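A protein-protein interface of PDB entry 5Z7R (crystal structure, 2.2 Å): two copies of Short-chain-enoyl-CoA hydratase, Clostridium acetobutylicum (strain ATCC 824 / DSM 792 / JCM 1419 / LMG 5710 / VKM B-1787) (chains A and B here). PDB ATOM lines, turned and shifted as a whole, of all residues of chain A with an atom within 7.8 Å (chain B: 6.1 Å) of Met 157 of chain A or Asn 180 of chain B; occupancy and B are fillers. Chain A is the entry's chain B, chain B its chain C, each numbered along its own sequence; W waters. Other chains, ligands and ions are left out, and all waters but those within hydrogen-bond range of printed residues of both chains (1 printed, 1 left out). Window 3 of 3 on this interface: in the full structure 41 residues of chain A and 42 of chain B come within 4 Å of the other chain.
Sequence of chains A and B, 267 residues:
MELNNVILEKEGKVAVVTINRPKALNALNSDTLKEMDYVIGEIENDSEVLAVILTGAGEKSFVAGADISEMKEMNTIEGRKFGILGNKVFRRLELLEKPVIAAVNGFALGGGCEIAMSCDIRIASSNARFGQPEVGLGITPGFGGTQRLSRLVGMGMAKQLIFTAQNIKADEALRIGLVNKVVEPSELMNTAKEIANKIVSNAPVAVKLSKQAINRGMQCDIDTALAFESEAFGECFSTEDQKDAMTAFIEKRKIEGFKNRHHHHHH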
ATOM      1  N   LEU A 149      19.761  -9.124  32.986  1.00  0.00           N
ATOM      2  CA  LEU A 149      20.659 -10.240  32.921  1.00  0.00           C
ATOM      3  C   LEU A 149      21.898  -9.953  32.066  1.00  0.00           C
ATOM      4  O   LEU A 149      22.975 -10.131  32.548  1.00  0.00           O
ATOM      5  CB  LEU A 149      19.915 -11.468  32.453  1.00  0.00           C
ATOM      6  CG  LEU A 149      20.725 -12.768  32.429  1.00  0.00           C
ATOM      7  CD1 LEU A 149      21.280 -13.149  33.780  1.00  0.00           C
ATOM      8  CD2 LEU A 149      19.824 -13.877  31.907  1.00  0.00           C
ATOM      9  N   SER A 150      21.742  -9.494  30.828  1.00  0.00           N
ATOM     10  CA  SER A 150      22.888  -9.149  30.032  1.00  0.00           C
ATOM     11  C   SER A 150      23.741  -8.085  30.734  1.00  0.00           C
ATOM     12  O   SER A 150      24.965  -8.174  30.710  1.00  0.00           O
ATOM     13  CB  SER A 150      22.492  -8.674  28.622  1.00  0.00           C
ATOM     14  OG  SER A 150      21.396  -7.790  28.674  1.00  0.00           O
ATOM     15  N   LEU A 152      24.071  -7.625  33.807  1.00  0.00           N
ATOM     16  CA  LEU A 152      24.685  -8.164  35.010  1.00  0.00           C
ATOM     17  C   LEU A 152      25.762  -9.219  34.741  1.00  0.00           C
ATOM     18  O   LEU A 152      26.767  -9.247  35.453  1.00  0.00           O
ATOM     19  CB  LEU A 152      23.624  -8.720  35.957  1.00  0.00           C
ATOM     20  CG  LEU A 152      23.157  -7.852  37.135  1.00  0.00           C
ATOM     21  CD1 LEU A 152      23.663  -6.402  37.100  1.00  0.00           C
ATOM     22  CD2 LEU A 152      21.647  -7.921  37.265  1.00  0.00           C
ATOM     23  N   VAL A 153      25.554 -10.083  33.743  1.00  0.00           N
ATOM     24  CA  VAL A 153      26.520 -11.159  33.434  1.00  0.00           C
ATOM     25  C   VAL A 153      27.037 -11.174  31.984  1.00  0.00           C
ATOM     26  O   VAL A 153      27.667 -12.145  31.559  1.00  0.00           O
ATOM     27  CB  VAL A 153      25.915 -12.532  33.798  1.00  0.00           C
ATOM     28  CG1 VAL A 153      25.240 -12.481  35.167  1.00  0.00           C
ATOM     29  CG2 VAL A 153      24.897 -12.989  32.777  1.00  0.00           C
ATOM     30  N   GLY A 154      26.772 -10.137  31.206  1.00  0.00           N
ATOM     31  CA  GLY A 154      27.264 -10.117  29.816  1.00  0.00           C
ATOM     32  C   GLY A 154      26.293 -10.752  28.830  1.00  0.00           C
ATOM     33  O   GLY A 154      25.447 -11.570  29.221  1.00  0.00           O
ATOM     34  N   MET A 155      26.401 -10.363  27.569  1.00  0.00           N
ATOM     35  CA  MET A 155      25.483 -10.823  26.513  1.00  0.00           C
ATOM     36  C   MET A 155      25.529 -12.307  26.226  1.00  0.00           C
ATOM     37  O   MET A 155      24.512 -12.936  25.936  1.00  0.00           O
ATOM     38  CB  MET A 155      25.736 -10.060  25.204  1.00  0.00           C
ATOM     39  CG  MET A 155      25.068  -8.700  25.204  1.00  0.00           C
ATOM     40  SD  MET A 155      24.143  -8.319  23.688  1.00  0.00           S
ATOM     41  CE  MET A 155      25.491  -8.306  22.488  1.00  0.00           C
ATOM     42  N   GLY A 156      26.742 -12.838  26.270  1.00  0.00           N
ATOM     43  CA  GLY A 156      27.018 -14.238  26.005  1.00  0.00           C
ATOM     44  C   GLY A 156      26.263 -15.168  26.908  1.00  0.00           C
ATOM     45  O   GLY A 156      25.579 -16.081  26.404  1.00  0.00           O
ATOM     46  N   MET A 157      26.365 -14.957  28.233  1.00  0.00           N
ATOM     47  CA  MET A 157      25.674 -15.823  29.158  1.00  0.00           C
ATOM     48  C   MET A 157      24.192 -15.522  29.168  1.00  0.00           C
ATOM     49  O   MET A 157      23.377 -16.444  29.196  1.00  0.00           O
ATOM     50  CB  MET A 157      26.191 -15.677  30.593  1.00  0.00           C
ATOM     51  CG  MET A 157      27.161 -16.728  31.074  1.00  0.00           C
ATOM     52  SD  MET A 157      26.728 -18.439  30.680  1.00  0.00           S
ATOM     53  CE  MET A 157      25.669 -18.827  32.061  1.00  0.00           C
ATOM     54  N   ALA A 158      23.829 -14.233  29.205  1.00  0.00           N
ATOM     55  CA  ALA A 158      22.399 -13.865  29.203  1.00  0.00           C
ATOM     56  C   ALA A 158      21.654 -14.547  28.053  1.00  0.00           C
ATOM     57  O   ALA A 158      20.605 -15.125  28.233  1.00  0.00           O
ATOM     58  CB  ALA A 158      22.219 -12.365  29.106  1.00  0.00           C
ATOM     59  N   LYS A 159      22.215 -14.449  26.868  1.00  0.00           N
ATOM     60  CA  LYS A 159      21.571 -15.020  25.707  1.00  0.00           C
ATOM     61  C   LYS A 159      21.392 -16.529  25.861  1.00  0.00           C
ATOM     62  O   LYS A 159      20.328 -17.071  25.564  1.00  0.00           O
ATOM     63  CB  LYS A 159      22.328 -14.657  24.432  1.00  0.00           C
ATOM     64  CG  LYS A 159      21.985 -13.286  23.896  1.00  0.00           C
ATOM     65  CD  LYS A 159      22.884 -12.868  22.747  1.00  0.00           C
ATOM     66  CE  LYS A 159      22.575 -11.459  22.256  1.00  0.00           C
ATOM     67  NZ  LYS A 159      23.167 -11.082  20.927  1.00  0.00           N
ATOM     68  N   GLN A 160      22.403 -17.199  26.379  1.00  0.00           N
ATOM     69  CA  GLN A 160      22.318 -18.635  26.512  1.00  0.00           C
ATOM     70  C   GLN A 160      21.203 -19.010  27.489  1.00  0.00           C
ATOM     71  O   GLN A 160      20.372 -19.905  27.213  1.00  0.00           O
ATOM     72  CB  GLN A 160      23.667 -19.228  26.967  1.00  0.00           C
ATOM     73  CG  GLN A 160      23.717 -20.747  26.914  1.00  0.00           C
ATOM     74  CD  GLN A 160      25.095 -21.307  27.182  1.00  0.00           C
ATOM     75  OE1 GLN A 160      26.026 -21.166  26.369  1.00  0.00           O
ATOM     76  NE2 GLN A 160      25.243 -21.944  28.348  1.00  0.00           N
ATOM     77  N   LEU A 161      21.165 -18.330  28.628  1.00  0.00           N
ATOM     78  CA  LEU A 161      20.215 -18.678  29.655  1.00  0.00           C
ATOM     79  C   LEU A 161      18.809 -18.396  29.181  1.00  0.00           C
ATOM     80  O   LEU A 161      17.882 -19.188  29.444  1.00  0.00           O
ATOM     81  CB  LEU A 161      20.480 -17.908  30.934  1.00  0.00           C
ATOM     82  CG  LEU A 161      21.481 -18.456  31.957  1.00  0.00           C
ATOM     83  CD1 LEU A 161      22.399 -19.501  31.353  1.00  0.00           C
ATOM     84  CD2 LEU A 161      22.299 -17.332  32.578  1.00  0.00           C
ATOM     85  N   ILE A 162      18.654 -17.280  28.491  1.00  0.00           N
ATOM     86  CA  ILE A 162      17.355 -16.894  28.014  1.00  0.00           C
ATOM     87  C   ILE A 162      16.891 -17.774  26.820  1.00  0.00           C
ATOM     88  O   ILE A 162      15.736 -18.162  26.808  1.00  0.00           O
ATOM     89  CB  ILE A 162      17.284 -15.385  27.717  1.00  0.00           C
ATOM     90  CG1 ILE A 162      17.295 -14.616  29.036  1.00  0.00           C
ATOM     91  CG2 ILE A 162      16.031 -15.014  26.933  1.00  0.00           C
ATOM     92  CD1 ILE A 162      17.449 -13.108  28.877  1.00  0.00           C
ATOM     93  N   PHE A 163      17.749 -18.062  25.835  1.00  0.00           N
ATOM     94  CA  PHE A 163      17.341 -18.877  24.695  1.00  0.00           C
ATOM     95  C   PHE A 163      17.148 -20.343  25.045  1.00  0.00           C
ATOM     96  O   PHE A 163      16.288 -20.978  24.487  1.00  0.00           O
ATOM     97  CB  PHE A 163      18.321 -18.817  23.518  1.00  0.00           C
ATOM     98  CG  PHE A 163      18.647 -17.438  23.012  1.00  0.00           C
ATOM     99  CD1 PHE A 163      17.777 -16.361  23.167  1.00  0.00           C
ATOM    100  CD2 PHE A 163      19.815 -17.242  22.302  1.00  0.00           C
ATOM    101  CE1 PHE A 163      18.103 -15.111  22.668  1.00  0.00           C
ATOM    102  CE2 PHE A 163      20.134 -16.011  21.788  1.00  0.00           C
ATOM    103  CZ  PHE A 163      19.278 -14.938  21.971  1.00  0.00           C
ATOM    104  N   THR A 164      17.940 -20.891  25.944  1.00  0.00           N
ATOM    105  CA  THR A 164      17.760 -22.288  26.348  1.00  0.00           C
ATOM    106  C   THR A 164      16.697 -22.529  27.441  1.00  0.00           C
ATOM    107  O   THR A 164      16.125 -23.609  27.493  1.00  0.00           O
ATOM    108  CB  THR A 164      19.044 -22.892  26.909  1.00  0.00           C
ATOM    109  OG1 THR A 164      19.398 -22.208  28.103  1.00  0.00           O
ATOM    110  CG2 THR A 164      20.178 -22.860  25.898  1.00  0.00           C
ATOM    111  N   GLN A 166      17.341 -22.951  30.442  1.00  0.00           N
ATOM    112  CA  GLN A 166      17.892 -23.860  31.418  1.00  0.00           C
ATOM    113  C   GLN A 166      18.489 -23.150  32.610  1.00  0.00           C
ATOM    114  O   GLN A 166      19.251 -22.210  32.458  1.00  0.00           O
ATOM    115  CB  GLN A 166      18.933 -24.747  30.769  1.00  0.00           C
ATOM    116  CG  GLN A 166      18.322 -25.528  29.620  1.00  0.00           C
ATOM    117  CD  GLN A 166      19.151 -26.715  29.185  1.00  0.00           C
ATOM    118  OE1 GLN A 166      18.826 -27.858  29.534  1.00  0.00           O
ATOM    119  NE2 GLN A 166      20.214 -26.459  28.402  1.00  0.00           N
ATOM    120  N   ILE A 168      20.735 -22.873  36.308  1.00  0.00           N
ATOM    121  CA  ILE A 168      22.150 -22.972  36.685  1.00  0.00           C
ATOM    122  C   ILE A 168      22.154 -22.995  38.182  1.00  0.00           C
ATOM    123  O   ILE A 168      21.265 -22.423  38.795  1.00  0.00           O
ATOM    124  CB  ILE A 168      23.018 -21.770  36.196  1.00  0.00           C
ATOM    125  CG1 ILE A 168      22.527 -20.433  36.772  1.00  0.00           C
ATOM    126  CG2 ILE A 168      23.056 -21.686  34.678  1.00  0.00           C
ATOM    127  CD1 ILE A 168      23.496 -19.273  36.578  1.00  0.00           C
ATOM    128  N   GLU A 172      27.637 -21.638  39.828  1.00  0.00           N
ATOM    129  CA  GLU A 172      27.774 -21.113  38.471  1.00  0.00           C
ATOM    130  C   GLU A 172      27.284 -19.670  38.445  1.00  0.00           C
ATOM    131  O   GLU A 172      27.851 -18.835  37.739  1.00  0.00           O
ATOM    132  CB  GLU A 172      26.946 -21.965  37.502  1.00  0.00           C
ATOM    133  CG  GLU A 172      26.929 -21.511  36.046  1.00  0.00           C
ATOM    134  CD  GLU A 172      28.264 -21.647  35.360  1.00  0.00           C
ATOM    135  OE1 GLU A 172      28.326 -21.290  34.164  1.00  0.00           O
ATOM    136  OE2 GLU A 172      29.259 -22.073  36.008  1.00  0.00           O
ATOM    137  N   ALA A 173      26.222 -19.379  39.188  1.00  0.00           N
ATOM    138  CA  ALA A 173      25.756 -17.990  39.320  1.00  0.00           C
ATOM    139  C   ALA A 173      26.876 -17.095  39.851  1.00  0.00           C
ATOM    140  O   ALA A 173      27.011 -15.950  39.421  1.00  0.00           O
ATOM    141  CB  ALA A 173      24.545 -17.890  40.198  1.00  0.00           C
ATOM    142  N   ARG A 175      30.202 -17.817  39.432  1.00  0.00           N
ATOM    143  CA  ARG A 175      31.286 -17.741  38.428  1.00  0.00           C
ATOM    144  C   ARG A 175      31.022 -16.646  37.384  1.00  0.00           C
ATOM    145  O   ARG A 175      31.954 -16.012  36.885  1.00  0.00           O
ATOM    146  CB  ARG A 175      31.501 -19.109  37.754  1.00  0.00           C
ATOM    147  CG  ARG A 175      32.499 -19.138  36.604  1.00  0.00           C
ATOM    148  CD  ARG A 175      32.460 -20.464  35.846  1.00  0.00           C
ATOM    149  NE  ARG A 175      31.430 -20.510  34.786  1.00  0.00           N
ATOM    150  CZ  ARG A 175      31.480 -19.799  33.650  1.00  0.00           C
ATOM    151  NH1 ARG A 175      32.498 -18.993  33.381  1.00  0.00           N
ATOM    152  NH2 ARG A 175      30.508 -19.897  32.770  1.00  0.00           N
ATOM    153  N   ILE A 176      29.760 -16.442  37.032  1.00  0.00           N
ATOM    154  CA  ILE A 176      29.441 -15.447  35.998  1.00  0.00           C
ATOM    155  C   ILE A 176      29.087 -14.086  36.600  1.00  0.00           C
ATOM    156  O   ILE A 176      28.737 -13.165  35.881  1.00  0.00           O
ATOM    157  CB  ILE A 176      28.284 -15.908  35.108  1.00  0.00           C
ATOM    158  CG1 ILE A 176      27.016 -16.092  35.936  1.00  0.00           C
ATOM    159  CG2 ILE A 176      28.700 -17.177  34.394  1.00  0.00           C
ATOM    160  CD1 ILE A 176      25.789 -16.320  35.114  1.00  0.00           C
ATOM    161  N   GLY A 177      29.116 -13.994  37.924  1.00  0.00           N
ATOM    162  CA  GLY A 177      28.998 -12.723  38.619  1.00  0.00           C
ATOM    163  C   GLY A 177      27.563 -12.321  38.906  1.00  0.00           C
ATOM    164  O   GLY A 177      27.317 -11.178  39.239  1.00  0.00           O
ATOM    165  N   ASP B 120      25.845 -15.002  19.042  1.00  0.00           N
ATOM    166  CA  ASP B 120      25.105 -14.787  20.254  1.00  0.00           C
ATOM    167  C   ASP B 120      25.774 -15.486  21.409  1.00  0.00           C
ATOM    168  O   ASP B 120      25.706 -15.047  22.572  1.00  0.00           O
ATOM    169  CB  ASP B 120      23.678 -15.392  20.099  1.00  0.00           C
ATOM    170  CG  ASP B 120      22.796 -14.618  19.116  1.00  0.00           C
ATOM    171  OD1 ASP B 120      22.458 -13.439  19.396  1.00  0.00           O
ATOM    172  OD2 ASP B 120      22.424 -15.172  18.049  1.00  0.00           O
ATOM    173  N   ILE B 121      26.327 -16.653  21.102  1.00  0.00           N
ATOM    174  CA  ILE B 121      26.897 -17.562  22.091  1.00  0.00           C
ATOM    175  C   ILE B 121      28.205 -18.199  21.568  1.00  0.00           C
ATOM    176  O   ILE B 121      28.302 -18.630  20.406  1.00  0.00           O
ATOM    177  CB  ILE B 121      25.894 -18.672  22.422  1.00  0.00           C
ATOM    178  CG1 ILE B 121      24.653 -18.070  23.073  1.00  0.00           C
ATOM    179  CG2 ILE B 121      26.516 -19.711  23.351  1.00  0.00           C
ATOM    180  CD1 ILE B 121      23.413 -18.912  22.925  1.00  0.00           C
ATOM    181  N   ARG B 122      29.221 -18.203  22.410  1.00  0.00           N
ATOM    182  CA  ARG B 122      30.521 -18.781  22.059  1.00  0.00           C
ATOM    183  C   ARG B 122      30.821 -19.907  23.051  1.00  0.00           C
ATOM    184  O   ARG B 122      30.805 -19.732  24.235  1.00  0.00           O
ATOM    185  CB  ARG B 122      31.650 -17.748  22.072  1.00  0.00           C
ATOM    186  CG  ARG B 122      31.754 -16.880  20.813  1.00  0.00           C
ATOM    187  CD  ARG B 122      32.372 -15.514  21.156  1.00  0.00           C
ATOM    188  NE  ARG B 122      31.580 -14.888  22.221  1.00  0.00           N
ATOM    189  CZ  ARG B 122      30.420 -14.303  22.017  1.00  0.00           C
ATOM    190  NH1 ARG B 122      29.751 -13.838  23.039  1.00  0.00           N
ATOM    191  NH2 ARG B 122      29.918 -14.205  20.796  1.00  0.00           N
ATOM    192  N   ILE B 123      31.111 -21.061  22.488  1.00  0.00           N
ATOM    193  CA  ILE B 123      31.476 -22.230  23.186  1.00  0.00           C
ATOM    194  C   ILE B 123      32.841 -22.586  22.552  1.00  0.00           C
ATOM    195  O   ILE B 123      33.060 -22.295  21.385  1.00  0.00           O
ATOM    196  CB  ILE B 123      30.317 -23.252  22.986  1.00  0.00           C
ATOM    197  CG1 ILE B 123      29.748 -23.678  24.327  1.00  0.00           C
ATOM    198  CG2 ILE B 123      30.672 -24.451  22.157  1.00  0.00           C
ATOM    199  CD1 ILE B 123      28.750 -22.680  24.870  1.00  0.00           C
ATOM    200  N   ALA B 124      33.751 -23.193  23.305  1.00  0.00           N
ATOM    201  CA  ALA B 124      35.070 -23.507  22.767  1.00  0.00           C
ATOM    202  C   ALA B 124      35.618 -24.895  23.128  1.00  0.00           C
ATOM    203  O   ALA B 124      35.367 -25.408  24.208  1.00  0.00           O
ATOM    204  CB  ALA B 124      36.046 -22.441  23.213  1.00  0.00           C
ATOM    205  N   LEU B 174      37.380 -18.381  28.944  1.00  0.00           N
ATOM    206  CA  LEU B 174      36.292 -18.710  29.828  1.00  0.00           C
ATOM    207  C   LEU B 174      36.309 -17.808  31.049  1.00  0.00           C
ATOM    208  O   LEU B 174      35.247 -17.371  31.535  1.00  0.00           O
ATOM    209  CB  LEU B 174      36.429 -20.174  30.250  1.00  0.00           C
ATOM    210  CG  LEU B 174      35.423 -20.657  31.258  1.00  0.00           C
ATOM    211  CD1 LEU B 174      34.059 -20.751  30.582  1.00  0.00           C
ATOM    212  CD2 LEU B 174      35.890 -21.985  31.856  1.00  0.00           C
ATOM    213  N   GLY B 177      34.941 -14.492  30.329  1.00  0.00           N
ATOM    214  CA  GLY B 177      33.550 -14.511  29.829  1.00  0.00           C
ATOM    215  C   GLY B 177      33.404 -14.447  28.328  1.00  0.00           C
ATOM    216  O   GLY B 177      32.293 -14.402  27.813  1.00  0.00           O
ATOM    217  N   LEU B 178      34.523 -14.467  27.622  1.00  0.00           N
ATOM    218  CA  LEU B 178      34.501 -14.486  26.177  1.00  0.00           C
ATOM    219  C   LEU B 178      33.744 -15.720  25.603  1.00  0.00           C
ATOM    220  O   LEU B 178      33.238 -15.684  24.478  1.00  0.00           O
ATOM    221  CB  LEU B 178      35.939 -14.443  25.648  1.00  0.00           C
ATOM    222  CG  LEU B 178      36.021 -14.420  24.131  1.00  0.00           C
ATOM    223  CD1 LEU B 178      35.150 -13.319  23.494  1.00  0.00           C
ATOM    224  CD2 LEU B 178      37.458 -14.340  23.610  1.00  0.00           C
ATOM    225  N   VAL B 179      33.757 -16.823  26.357  1.00  0.00           N
ATOM    226  CA  VAL B 179      33.012 -18.025  26.019  1.00  0.00           C
ATOM    227  C   VAL B 179      32.303 -18.507  27.276  1.00  0.00           C
ATOM    228  O   VAL B 179      32.749 -18.243  28.413  1.00  0.00           O
ATOM    229  CB  VAL B 179      33.929 -19.151  25.501  1.00  0.00           C
ATOM    230  CG1 VAL B 179      34.643 -18.716  24.233  1.00  0.00           C
ATOM    231  CG2 VAL B 179      34.936 -19.603  26.566  1.00  0.00           C
ATOM    232  N   ASN B 180      31.186 -19.192  27.069  1.00  0.00           N
ATOM    233  CA  ASN B 180      30.352 -19.700  28.159  1.00  0.00           C
ATOM    234  C   ASN B 180      30.843 -21.031  28.671  1.00  0.00           C
ATOM    235  O   ASN B 180      30.561 -21.421  29.794  1.00  0.00           O
ATOM    236  CB  ASN B 180      28.924 -19.849  27.677  1.00  0.00           C
ATOM    237  CG  ASN B 180      28.334 -18.540  27.243  1.00  0.00           C
ATOM    238  OD1 ASN B 180      28.992 -17.501  27.311  1.00  0.00           O
ATOM    239  ND2 ASN B 180      27.121 -18.582  26.762  1.00  0.00           N
ATOM    240  N   LYS B 181      31.597 -21.736  27.853  1.00  0.00           N
ATOM    241  CA  LYS B 181      31.978 -23.120  28.212  1.00  0.00           C
ATOM    242  C   LYS B 181      33.167 -23.611  27.411  1.00  0.00           C
ATOM    243  O   LYS B 181      33.438 -23.148  26.297  1.00  0.00           O
ATOM    244  CB  LYS B 181      30.767 -24.074  28.051  1.00  0.00           C
ATOM    245  CG  LYS B 181      30.908 -25.387  28.820  1.00  0.00           C
ATOM    246  CD  LYS B 181      29.640 -26.216  28.770  1.00  0.00           C
ATOM    247  CE  LYS B 181      29.840 -27.561  29.463  1.00  0.00           C
ATOM    248  NZ  LYS B 181      28.511 -28.195  29.723  1.00  0.00           N
ATOM    249  N   VAL B 182      33.894 -24.549  27.998  1.00  0.00           N
ATOM    250  CA  VAL B 182      35.027 -25.178  27.316  1.00  0.00           C
ATOM    251  C   VAL B 182      34.954 -26.664  27.538  1.00  0.00           C
ATOM    252  O   VAL B 182      34.685 -27.108  28.646  1.00  0.00           O
ATOM    253  CB  VAL B 182      36.353 -24.634  27.828  1.00  0.00           C
ATOM    254  CG1 VAL B 182      37.528 -25.396  27.233  1.00  0.00           C
ATOM    255  CG2 VAL B 182      36.447 -23.154  27.509  1.00  0.00           C
HETATM  256  O   HOH W   1      35.178 -18.376  34.349  1.00  0.00           O
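The backbone carbonyl oxygen of Gly 156 of chain A lies within hydrogen-bond range of the side-chain amide nitrogen of Asn 180 of chain B (3.0 Å). The side-chain carboxylate (OD1) of Asp 120 of chain B is in salt-bridge range of the side-chain amino group (NZ) of Lys 159 of chain A, 2.9 Å away. OE1 of Gln 160 of chain A lies within hydrogen-bond range of ND2 of Asn 180 of chain B (2.8 Å). The guanidinium group of Arg 175 of chain A sits at hydrogen-bond distance from the backbone carbonyl oxygen of Asn 180 of chain B, 3.3 Å away.
OG1 of Thr 164 of chain A sits at hydrogen-bond distance from O of Gln 160 of chain A (2.7 Å). The side-chain carboxylate (OE1) of Glu 172 of chain A lies within salt-bridge range of the guanidinium group (NH2) of Arg 175 of chain A (2.9 Å). The backbone carbonyl oxygen (O) of Arg 122 of chain B is in hydrogen-bond range of the backbone NH (N) of Asn 180 of chain B (2.9 Å).
Among the printed residues, merely in contact across the chains: Gln 160 of chain A with Ile 121 of chain B (3.4 Å), Gln 160 of chain A with Ile 123 of chain B (3.5 Å), Arg 175 of chain A with Leu 174 of chain B (3.7 Å), Gly 156 of chain A with Asp 120 of chain B (3.8 Å), Met 157 of chain A with Asn 180 of chain B (3.8 Å), Phe 163 of chain A with Asp 120 of chain B (3.97 Å) and Gly 156 of chain A with Ile 121 of chain B (3.99 Å).
Of chain B, only Asn 180 comes within 4 Å of Met 157 of chain A. Printed residues of chain B within 4 Å of Gln 160 of chain A: Ile 121, Ile 123 and Asn 180. Of the printed residues of chain B, Phe 163 of chain A touches Asp 120 (3.97 Å). Of the printed residues of chain A, Ile 121 of chain B touches Gly 156 (3.99 Å) and Gln 160 (3.4 Å). Printed residues of chain A within 4 Å of Ile 123 of chain B: Gln 160. Printed residues of chain A within 4 Å of Leu 174 of chain B: Arg 175 (3.7 Å). Of chain A, only Gly 156 (3.0 Å), Met 157 (3.8 Å), Gln 160 (2.8 Å) and Arg 175 (3.3 Å) come within 4 Å of Asn 180 of chain B. The nearest residue of chain B that does not touch Met 157 of chain A is Asp 120 of chain B (5.7 Å). The nearest residue of chain A that does not touch Asn 180 of chain B is Glu 172 of chain A (4.9 Å).
Of the 22 printed residues of chain A, 6 touch a printed residue of chain B. Among the printed residues, 11 pairs touch across the chains. Among the printed residues, Asp or Glu carboxylates within 4 Å of a Lys or Arg side-chain nitrogen of the other chain: Lys 159 of chain A with Asp 120 of chain B (2.9 Å).
1 position is printed for both chains. Of the 11 pairs that touch across the chains among the printed residues, none has its exchanged pair printed and touching as well.
Water W1 bridges NH1 of Arg 175 of chain A (2.9 Å) and O of Leu 174 of chain B (3.0 Å).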
